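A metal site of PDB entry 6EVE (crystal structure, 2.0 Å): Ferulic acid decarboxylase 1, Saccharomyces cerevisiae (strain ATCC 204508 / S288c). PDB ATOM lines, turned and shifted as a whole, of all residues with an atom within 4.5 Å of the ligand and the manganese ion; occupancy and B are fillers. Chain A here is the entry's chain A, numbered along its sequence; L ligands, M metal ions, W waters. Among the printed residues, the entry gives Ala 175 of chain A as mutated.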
ATOM      1  N   THR A 155      22.023 -15.512   9.326  1.00  0.00           N
ATOM      2  CA  THR A 155      21.966 -16.763   8.589  1.00  0.00           C
ATOM      3  C   THR A 155      21.251 -17.942   9.332  1.00  0.00           C
ATOM      4  O   THR A 155      20.984 -18.978   8.721  1.00  0.00           O
ATOM      5  CB  THR A 155      23.352 -17.264   8.237  1.00  0.00           C
ATOM      6  OG1 THR A 155      24.135 -17.465   9.433  1.00  0.00           O
ATOM      7  CG2 THR A 155      24.078 -16.261   7.314  1.00  0.00           C
ATOM      8  N   TYR A 156      20.958 -17.794  10.625  1.00  0.00           N
ATOM      9  CA  TYR A 156      20.327 -18.891  11.410  1.00  0.00           C
ATOM     10  C   TYR A 156      19.557 -18.448  12.623  1.00  0.00           C
ATOM     11  O   TYR A 156      19.526 -19.161  13.637  1.00  0.00           O
ATOM     12  CB  TYR A 156      21.381 -19.919  11.882  1.00  0.00           C
ATOM     13  CG  TYR A 156      20.857 -21.348  12.023  1.00  0.00           C
ATOM     14  CD1 TYR A 156      20.574 -22.111  10.903  1.00  0.00           C
ATOM     15  CD2 TYR A 156      20.662 -21.928  13.272  1.00  0.00           C
ATOM     16  CE1 TYR A 156      20.080 -23.438  11.011  1.00  0.00           C
ATOM     17  CE2 TYR A 156      20.194 -23.261  13.400  1.00  0.00           C
ATOM     18  CZ  TYR A 156      19.922 -24.017  12.262  1.00  0.00           C
ATOM     19  OH  TYR A 156      19.462 -25.327  12.386  1.00  0.00           O
ATOM     20  N   TRP A 168      -2.270 -13.819  12.971  1.00  0.00           N
ATOM     21  CA  TRP A 168      -1.214 -14.665  12.434  1.00  0.00           C
ATOM     22  C   TRP A 168       0.162 -14.079  12.791  1.00  0.00           C
ATOM     23  O   TRP A 168       0.441 -12.904  12.512  1.00  0.00           O
ATOM     24  CB  TRP A 168      -1.462 -14.807  10.937  1.00  0.00           C
ATOM     25  CG  TRP A 168      -0.416 -15.613  10.177  1.00  0.00           C
ATOM     26  CD1 TRP A 168       0.434 -16.555  10.661  1.00  0.00           C
ATOM     27  CD2 TRP A 168      -0.113 -15.491   8.786  1.00  0.00           C
ATOM     28  NE1 TRP A 168       1.225 -17.049   9.669  1.00  0.00           N
ATOM     29  CE2 TRP A 168       0.917 -16.407   8.506  1.00  0.00           C
ATOM     30  CE3 TRP A 168      -0.654 -14.727   7.740  1.00  0.00           C
ATOM     31  CZ2 TRP A 168       1.444 -16.563   7.235  1.00  0.00           C
ATOM     32  CZ3 TRP A 168      -0.170 -14.897   6.476  1.00  0.00           C
ATOM     33  CH2 TRP A 168       0.878 -15.820   6.221  1.00  0.00           C
ATOM     34  N   ASN A 170       4.070 -15.040  12.101  1.00  0.00           N
ATOM     35  CA  ASN A 170       4.975 -15.891  11.325  1.00  0.00           C
ATOM     36  C   ASN A 170       6.413 -15.864  11.888  1.00  0.00           C
ATOM     37  O   ASN A 170       6.965 -14.782  12.193  1.00  0.00           O
ATOM     38  CB  ASN A 170       4.940 -15.482   9.861  1.00  0.00           C
ATOM     39  CG  ASN A 170       5.422 -16.546   8.922  1.00  0.00           C
ATOM     40  OD1 ASN A 170       6.623 -16.570   8.494  1.00  0.00           O
ATOM     41  ND2 ASN A 170       4.539 -17.443   8.579  1.00  0.00           N
ATOM     42  N   TRP A 171       7.006 -17.070  12.020  1.00  0.00           N
ATOM     43  CA  TRP A 171       8.440 -17.284  12.336  1.00  0.00           C
ATOM     44  C   TRP A 171       9.127 -17.856  11.060  1.00  0.00           C
ATOM     45  O   TRP A 171       8.637 -18.835  10.483  1.00  0.00           O
ATOM     46  CB  TRP A 171       8.588 -18.299  13.473  1.00  0.00           C
ATOM     47  CG  TRP A 171       8.080 -17.860  14.838  1.00  0.00           C
ATOM     48  CD1 TRP A 171       7.634 -16.616  15.174  1.00  0.00           C
ATOM     49  CD2 TRP A 171       8.127 -18.615  16.067  1.00  0.00           C
ATOM     50  NE1 TRP A 171       7.383 -16.556  16.501  1.00  0.00           N
ATOM     51  CE2 TRP A 171       7.656 -17.760  17.089  1.00  0.00           C
ATOM     52  CE3 TRP A 171       8.464 -19.924  16.399  1.00  0.00           C
ATOM     53  CZ2 TRP A 171       7.499 -18.177  18.429  1.00  0.00           C
ATOM     54  CZ3 TRP A 171       8.324 -20.348  17.765  1.00  0.00           C
ATOM     55  CH2 TRP A 171       7.874 -19.467  18.747  1.00  0.00           C
ATOM     56  N   SER A 172      10.212 -17.261  10.582  1.00  0.00           N
ATOM     57  CA  SER A 172      10.915 -17.764   9.388  1.00  0.00           C
ATOM     58  C   SER A 172      12.382 -17.350   9.291  1.00  0.00           C
ATOM     59  O   SER A 172      12.799 -16.399   9.916  1.00  0.00           O
ATOM     60  CB  SER A 172      10.203 -17.285   8.114  1.00  0.00           C
ATOM     61  OG  SER A 172      10.344 -15.873   7.925  1.00  0.00           O
ATOM     62  N   ILE A 173      13.141 -18.072   8.458  1.00  0.00           N
ATOM     63  CA  ILE A 173      14.529 -17.690   8.134  1.00  0.00           C
ATOM     64  C   ILE A 173      14.671 -17.041   6.759  1.00  0.00           C
ATOM     65  O   ILE A 173      14.126 -17.554   5.728  1.00  0.00           O
ATOM     66  CB  ILE A 173      15.457 -18.901   8.203  1.00  0.00           C
ATOM     67  CG1 ILE A 173      15.241 -19.576   9.555  1.00  0.00           C
ATOM     68  CG2 ILE A 173      16.910 -18.472   7.909  1.00  0.00           C
ATOM     69  CD1 ILE A 173      16.109 -20.785   9.787  1.00  0.00           C
ATOM     70  N   ALA A 174      15.421 -15.945   6.753  1.00  0.00           N
ATOM     71  CA  ALA A 174      15.809 -15.220   5.499  1.00  0.00           C
ATOM     72  C   ALA A 174      17.119 -14.420   5.729  1.00  0.00           C
ATOM     73  O   ALA A 174      17.251 -13.818   6.770  1.00  0.00           O
ATOM     74  CB  ALA A 174      14.687 -14.297   5.042  1.00  0.00           C
ATOM     75  N   ALA A 175      18.069 -14.476   4.769  1.00  0.00           N
ATOM     76  CA  ALA A 175      19.426 -13.932   4.950  1.00  0.00           C
ATOM     77  C   ALA A 175      19.339 -12.440   5.219  1.00  0.00           C
ATOM     78  O   ALA A 175      18.509 -11.790   4.678  1.00  0.00           O
ATOM     79  CB  ALA A 175      20.339 -14.235   3.749  1.00  0.00           C
ATOM     80  N   GLN A 192       7.111 -15.936  -0.245  1.00  0.00           N
ATOM     81  CA  GLN A 192       7.414 -16.074   1.179  1.00  0.00           C
ATOM     82  C   GLN A 192       6.421 -15.287   2.103  1.00  0.00           C
ATOM     83  O   GLN A 192       5.946 -14.186   1.777  1.00  0.00           O
ATOM     84  CB  GLN A 192       8.918 -15.734   1.447  1.00  0.00           C
ATOM     85  CG  GLN A 192       9.941 -16.569   0.596  1.00  0.00           C
ATOM     86  CD  GLN A 192       9.991 -18.090   0.911  1.00  0.00           C
ATOM     87  OE1 GLN A 192       8.990 -18.809   0.628  1.00  0.00           O
ATOM     88  NE2 GLN A 192      11.138 -18.592   1.487  1.00  0.00           N
ATOM     89  N   HIS A 193       6.136 -15.872   3.255  1.00  0.00           N
ATOM     90  CA  HIS A 193       5.133 -15.355   4.189  1.00  0.00           C
ATOM     91  C   HIS A 193       5.525 -14.028   4.821  1.00  0.00           C
ATOM     92  O   HIS A 193       4.663 -13.227   5.138  1.00  0.00           O
ATOM     93  CB  HIS A 193       4.774 -16.408   5.252  1.00  0.00           C
ATOM     94  CG  HIS A 193       3.965 -17.546   4.707  1.00  0.00           C
ATOM     95  ND1 HIS A 193       3.762 -18.728   5.400  1.00  0.00           N
ATOM     96  CD2 HIS A 193       3.316 -17.695   3.528  1.00  0.00           C
ATOM     97  CE1 HIS A 193       3.026 -19.549   4.658  1.00  0.00           C
ATOM     98  NE2 HIS A 193       2.733 -18.941   3.531  1.00  0.00           N
ATOM     99  N   ILE A 194       6.817 -13.812   4.995  1.00  0.00           N
ATOM    100  CA  ILE A 194       7.312 -12.533   5.486  1.00  0.00           C
ATOM    101  C   ILE A 194       6.865 -11.363   4.570  1.00  0.00           C
ATOM    102  O   ILE A 194       6.428 -10.317   5.057  1.00  0.00           O
ATOM    103  CB  ILE A 194       8.839 -12.609   5.778  1.00  0.00           C
ATOM    104  CG1 ILE A 194       9.350 -11.337   6.382  1.00  0.00           C
ATOM    105  CG2 ILE A 194       9.633 -12.858   4.516  1.00  0.00           C
ATOM    106  CD1 ILE A 194      10.750 -11.538   6.935  1.00  0.00           C
ATOM    107  N   SER A 226      10.934 -22.725  11.554  1.00  0.00           N
ATOM    108  CA  SER A 226      11.170 -21.520  10.823  1.00  0.00           C
ATOM    109  C   SER A 226      11.572 -21.755   9.326  1.00  0.00           C
ATOM    110  O   SER A 226      11.219 -20.916   8.457  1.00  0.00           O
ATOM    111  CB  SER A 226      12.178 -20.622  11.581  1.00  0.00           C
ATOM    112  OG  SER A 226      11.612 -20.185  12.826  1.00  0.00           O
ATOM    113  N   SER A 227      12.275 -22.845   9.044  1.00  0.00           N
ATOM    114  CA  SER A 227      12.678 -23.192   7.695  1.00  0.00           C
ATOM    115  C   SER A 227      11.669 -24.088   6.955  1.00  0.00           C
ATOM    116  O   SER A 227      11.974 -24.564   5.858  1.00  0.00           O
ATOM    117  CB  SER A 227      13.989 -23.941   7.721  1.00  0.00           C
ATOM    118  OG  SER A 227      14.457 -24.200   6.389  1.00  0.00           O
ATOM    119  N   MET A 228      10.517 -24.371   7.582  1.00  0.00           N
ATOM    120  CA  MET A 228       9.513 -25.273   7.007  1.00  0.00           C
ATOM    121  C   MET A 228       8.319 -24.508   6.357  1.00  0.00           C
ATOM    122  O   MET A 228       7.793 -23.564   6.951  1.00  0.00           O
ATOM    123  CB  MET A 228       9.014 -26.193   8.113  1.00  0.00           C
ATOM    124  CG  MET A 228       7.964 -27.251   7.703  1.00  0.00           C
ATOM    125  SD  MET A 228       7.766 -28.417   9.114  1.00  0.00           S
ATOM    126  CE  MET A 228       6.585 -29.491   8.297  1.00  0.00           C
ATOM    127  N   PRO A 229       7.890 -24.905   5.152  1.00  0.00           N
ATOM    128  CA  PRO A 229       6.791 -24.235   4.521  1.00  0.00           C
ATOM    129  C   PRO A 229       5.420 -24.773   4.890  1.00  0.00           C
ATOM    130  O   PRO A 229       4.697 -25.402   4.063  1.00  0.00           O
ATOM    131  CB  PRO A 229       7.137 -24.371   3.023  1.00  0.00           C
ATOM    132  CG  PRO A 229       7.835 -25.682   2.942  1.00  0.00           C
ATOM    133  CD  PRO A 229       8.531 -25.890   4.241  1.00  0.00           C
ATOM    134  N   ILE A 230       5.017 -24.463   6.110  1.00  0.00           N
ATOM    135  CA  ILE A 230       3.664 -24.854   6.590  1.00  0.00           C
ATOM    136  C   ILE A 230       2.609 -23.886   5.987  1.00  0.00           C
ATOM    137  O   ILE A 230       2.961 -22.795   5.520  1.00  0.00           O
ATOM    138  CB  ILE A 230       3.578 -24.905   8.147  1.00  0.00           C
ATOM    139  CG1 ILE A 230       3.660 -23.519   8.792  1.00  0.00           C
ATOM    140  CG2 ILE A 230       4.680 -25.773   8.688  1.00  0.00           C
ATOM    141  CD1 ILE A 230       3.456 -23.536  10.304  1.00  0.00           C
ATOM    142  N   GLU A 236       3.582 -20.581  13.388  1.00  0.00           N
ATOM    143  CA  GLU A 236       4.577 -21.613  13.613  1.00  0.00           C
ATOM    144  C   GLU A 236       4.685 -21.972  15.118  1.00  0.00           C
ATOM    145  O   GLU A 236       4.809 -23.147  15.490  1.00  0.00           O
ATOM    146  CB  GLU A 236       5.971 -21.154  13.182  1.00  0.00           C
ATOM    147  CG  GLU A 236       6.335 -21.275  11.712  1.00  0.00           C
ATOM    148  CD  GLU A 236       5.647 -20.277  10.744  1.00  0.00           C
ATOM    149  OE1 GLU A 236       4.945 -19.342  11.186  1.00  0.00           O
ATOM    150  OE2 GLU A 236       5.873 -20.424   9.530  1.00  0.00           O
ATOM    151  N   SER A 317      25.022 -20.537   9.648  1.00  0.00           N
ATOM    152  CA  SER A 317      25.061 -21.344   8.461  1.00  0.00           C
ATOM    153  C   SER A 317      25.846 -20.636   7.290  1.00  0.00           C
ATOM    154  O   SER A 317      25.620 -19.448   7.018  1.00  0.00           O
ATOM    155  CB  SER A 317      23.620 -21.638   8.006  1.00  0.00           C
ATOM    156  OG  SER A 317      23.558 -22.425   6.835  1.00  0.00           O
ATOM    157  N   PRO A 319      26.294 -21.221   3.405  1.00  0.00           N
ATOM    158  CA  PRO A 319      25.781 -22.041   2.297  1.00  0.00           C
ATOM    159  C   PRO A 319      26.748 -22.259   1.148  1.00  0.00           C
ATOM    160  O   PRO A 319      27.510 -21.379   0.815  1.00  0.00           O
ATOM    161  CB  PRO A 319      24.564 -21.243   1.775  1.00  0.00           C
ATOM    162  CG  PRO A 319      24.270 -20.255   2.822  1.00  0.00           C
ATOM    163  CD  PRO A 319      25.574 -19.928   3.488  1.00  0.00           C
ATOM    164  N   GLU A 325      23.009 -26.569   5.859  1.00  0.00           N
ATOM    165  CA  GLU A 325      21.607 -26.414   6.257  1.00  0.00           C
ATOM    166  C   GLU A 325      20.621 -26.115   5.095  1.00  0.00           C
ATOM    167  O   GLU A 325      19.438 -26.448   5.173  1.00  0.00           O
ATOM    168  CB  GLU A 325      21.445 -25.356   7.345  1.00  0.00           C
ATOM    169  CG  GLU A 325      22.115 -25.705   8.660  1.00  0.00           C
ATOM    170  CD  GLU A 325      23.634 -25.541   8.700  1.00  0.00           C
ATOM    171  OE1 GLU A 325      24.189 -24.857   7.812  1.00  0.00           O
ATOM    172  OE2 GLU A 325      24.244 -26.139   9.616  1.00  0.00           O
ATOM    173  N   THR A 326      21.112 -25.521   4.014  1.00  0.00           N
ATOM    174  CA  THR A 326      20.257 -25.231   2.865  1.00  0.00           C
ATOM    175  C   THR A 326      19.893 -26.593   2.128  1.00  0.00           C
ATOM    176  O   THR A 326      19.080 -26.570   1.242  1.00  0.00           O
ATOM    177  CB  THR A 326      20.854 -24.124   1.925  1.00  0.00           C
ATOM    178  OG1 THR A 326      22.011 -24.607   1.220  1.00  0.00           O
ATOM    179  CG2 THR A 326      21.298 -22.873   2.694  1.00  0.00           C
ATOM    180  N   LEU A 329      17.970 -28.923   5.861  1.00  0.00           N
ATOM    181  CA  LEU A 329      16.720 -28.296   6.321  1.00  0.00           C
ATOM    182  C   LEU A 329      15.816 -27.840   5.172  1.00  0.00           C
ATOM    183  O   LEU A 329      14.665 -28.308   5.069  1.00  0.00           O
ATOM    184  CB  LEU A 329      16.954 -27.148   7.357  1.00  0.00           C
ATOM    185  CG  LEU A 329      17.695 -27.519   8.633  1.00  0.00           C
ATOM    186  CD1 LEU A 329      17.676 -26.290   9.540  1.00  0.00           C
ATOM    187  CD2 LEU A 329      17.033 -28.711   9.326  1.00  0.00           C
ATOM    188  N   ILE A 330      16.262 -26.940   4.307  1.00  0.00           N
ATOM    189  CA  ILE A 330      15.369 -26.418   3.270  1.00  0.00           C
ATOM    190  C   ILE A 330      14.842 -27.643   2.452  1.00  0.00           C
ATOM    191  O   ILE A 330      13.637 -27.791   2.234  1.00  0.00           O
ATOM    192  CB  ILE A 330      16.037 -25.395   2.317  1.00  0.00           C
ATOM    193  CG1 ILE A 330      16.529 -24.175   3.100  1.00  0.00           C
ATOM    194  CG2 ILE A 330      15.051 -24.989   1.220  1.00  0.00           C
ATOM    195  CD1 ILE A 330      17.298 -23.182   2.239  1.00  0.00           C
ATOM    196  N   LYS A 394       3.348 -23.054  -3.659  1.00  0.00           N
ATOM    197  CA  LYS A 394       4.500 -22.575  -2.914  1.00  0.00           C
ATOM    198  C   LYS A 394       5.549 -23.716  -2.534  1.00  0.00           C
ATOM    199  O   LYS A 394       6.724 -23.488  -2.583  1.00  0.00           O
ATOM    200  CB  LYS A 394       4.015 -21.826  -1.641  1.00  0.00           C
ATOM    201  CG  LYS A 394       5.140 -21.276  -0.750  1.00  0.00           C
ATOM    202  CD  LYS A 394       4.596 -20.299   0.301  1.00  0.00           C
ATOM    203  CE  LYS A 394       5.647 -19.906   1.332  1.00  0.00           C
ATOM    204  NZ  LYS A 394       5.863 -20.984   2.329  1.00  0.00           N
HETATM  205  C1  LIG L   1      16.531 -21.361   5.190  1.00  0.00           C
HETATM  206  C2  LIG L   1      17.629 -21.702   5.906  1.00  0.00           C
HETATM  207  C3  LIG L   1      18.865 -21.022   5.784  1.00  0.00           C
HETATM  208  C4  LIG L   1      15.465 -18.753   2.813  1.00  0.00           C
HETATM  209  C5  LIG L   1      18.996 -19.997   4.810  1.00  0.00           C
HETATM  210  N1  LIG L   1      15.358 -16.198   1.872  1.00  0.00           N
HETATM  211  C6  LIG L   1      14.229 -16.978   1.927  1.00  0.00           C
HETATM  212  C7  LIG L   1      21.543 -19.670   5.022  1.00  0.00           C
HETATM  213  C8  LIG L   1      20.200 -19.126   4.607  1.00  0.00           C
HETATM  214  C9  LIG L   1      19.182 -18.391   2.504  1.00  0.00           C
HETATM  215  O1  LIG L   1      13.060 -16.451   1.517  1.00  0.00           O
HETATM  216  N2  LIG L   1      14.265 -18.260   2.372  1.00  0.00           N
HETATM  217  C10 LIG L   1      16.595 -16.664   2.263  1.00  0.00           C
HETATM  218  O2  LIG L   1      17.548 -15.834   2.187  1.00  0.00           O
HETATM  219  C11 LIG L   1      16.695 -17.982   2.763  1.00  0.00           C
HETATM  220  N3  LIG L   1      17.902 -18.634   3.126  1.00  0.00           N
HETATM  221  C12 LIG L   1      20.341 -18.752   3.203  1.00  0.00           C
HETATM  222  C13 LIG L   1      19.959 -17.818   5.375  1.00  0.00           C
HETATM  223  C14 LIG L   1      17.835 -19.670   4.087  1.00  0.00           C
HETATM  224  C15 LIG L   1      20.035 -21.506   6.644  1.00  0.00           C
HETATM  225  C16 LIG L   1      17.433 -22.821   6.829  1.00  0.00           C
HETATM  226  C17 LIG L   1      16.588 -20.342   4.266  1.00  0.00           C
HETATM  227  N4  LIG L   1      15.424 -19.973   3.490  1.00  0.00           N
HETATM  228  C18 LIG L   1      14.132 -20.703   3.472  1.00  0.00           C
HETATM  229  C19 LIG L   1      12.952 -20.276   4.296  1.00  0.00           C
HETATM  230  O3  LIG L   1      13.393 -20.226   5.641  1.00  0.00           O
HETATM  231  C20 LIG L   1      11.833 -21.311   4.055  1.00  0.00           C
HETATM  232  O4  LIG L   1      11.424 -21.290   2.710  1.00  0.00           O
HETATM  233  C21 LIG L   1      10.597 -21.104   4.860  1.00  0.00           C
HETATM  234  O5  LIG L   1       9.540 -22.023   4.456  1.00  0.00           O
HETATM  235  C22 LIG L   1      10.070 -19.671   4.904  1.00  0.00           C
HETATM  236  O6  LIG L   1       9.013 -19.556   5.856  1.00  0.00           O
HETATM  237  P1  LIG L   1       7.458 -19.269   5.423  1.00  0.00           P
HETATM  238  O7  LIG L   1       6.729 -18.865   6.708  1.00  0.00           O
HETATM  239  O8  LIG L   1       7.618 -18.053   4.511  1.00  0.00           O
HETATM  240  O9  LIG L   1       6.936 -20.507   4.824  1.00  0.00           O
HETATM  241 MN    MN M   1       4.847 -19.424   7.569  1.00  0.00          MN
HETATM  242  O   HOH W   1       2.615 -20.049   8.105  1.00  0.00           O
HETATM  243  O   HOH W   2      11.150 -23.802   1.608  1.00  0.00           O
HETATM  244  O   HOH W   3       5.098 -21.451   6.524  1.00  0.00           O
HETATM  245  O   HOH W   4      11.943 -13.415   1.316  1.00  0.00           O
HETATM  246  O   HOH W   5      11.829 -16.297   4.101  1.00  0.00           O
HETATM  247  O   HOH W   6       9.046 -15.976   5.107  1.00  0.00           O
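NZ of Lys 394 lies within salt-bridge range of O9 of the ligand.
An oxygen (O5) of the ligand sits close to the backbone carbonyl oxygen of Met 228, 3.4 Å away.
N of Ala 175 is in hydrogen-bond range of O2 of the ligand, 3.0 Å away.
The backbone NH of His 193 is in hydrogen-bond range of an oxygen (O8) of the ligand (2.9 Å).
The side-chain amide nitrogen of Gln 192 sits at hydrogen-bond distance from an oxygen (O1) of the ligand.
The backbone carbonyl oxygen (O) of Ile 173 lies within hydrogen-bond range of an oxygen (O3) of the ligand (2.8 Å).
OE1 of Glu 236 is in hydrogen-bond range of N of Trp 171 (3.2 Å).
The side-chain carboxylate of Glu 325 lies within hydrogen-bond range of the side-chain hydroxyl of Ser 317 (2.7 Å).
The side-chain hydroxyl (OG1) of Thr 155 is in hydrogen-bond range of the backbone NH (N) of Ser 317 (3.2 Å).
The backbone NH of Ile 330 lies within hydrogen-bond range of the backbone carbonyl oxygen of Glu 325, 3.3 Å away.
N of Ile 173 is in hydrogen-bond range of O of Ser 226 (3.4 Å).
An oxygen (O5) of the ligand lies close to the backbone nitrogen of Pro 229, at 3.4 Å.
Merely in contact with the ligand: Ser 227 (3.3 Å), Thr 155 (3.4 Å), Ser 172 (3.4 Å), Ile 330 (3.5 Å), Pro 319 (3.6 Å), Ser 226 (3.6 Å), Ala 174 (3.6 Å), Ser 317 (3.6 Å) and Thr 326 (3.97 Å).
Hydrophobic or aromatic side chains within 4 Å of the ligand: Ile 173, Ala 174, Ala 175, His 193, Pro 229, Pro 319 and Ile 330.
18 residues have an atom within 4 Å of the ligand: Thr 155, Asn 170, Ser 172, Ile 173, Ala 174, Ala 175, Gln 192, His 193, Ser 226, Ser 227, Met 228, Pro 229, Glu 236, Ser 317, Pro 319, Thr 326, Ile 330 and Lys 394.
Within 4 Å of the manganese ion: Asn 170, His 193 and Glu 236.
The nearest printed residue that does not touch the manganese ion is Ile 230 (4.4 Å).
O7 of the ligand is bound to the manganese ion, at 2.1 Å.
The manganese ion is bound by ND2 of Asn 170.
Water W3 binds the manganese ion, at 2.3 Å.
Water W1 is bound to the manganese ion.
OE2 of Glu 236 binds the manganese ion, at 2.4 Å.
The manganese ion is bound by ND1 of His 193.
Water W3 lies within hydrogen-bond range of an oxygen (O9) of the ligand, the backbone carbonyl oxygen of Ile 230 and the backbone carbonyl oxygen of Met 228.
Water W6 lies within hydrogen-bond range of O8 of the ligand, OG of Ser 172, N of Ile 194 and N of His 193.
Water W5 bridges an oxygen (O1) of the ligand (2.9 Å) and the backbone carbonyl oxygen (O) of Ile 173 (3.1 Å).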
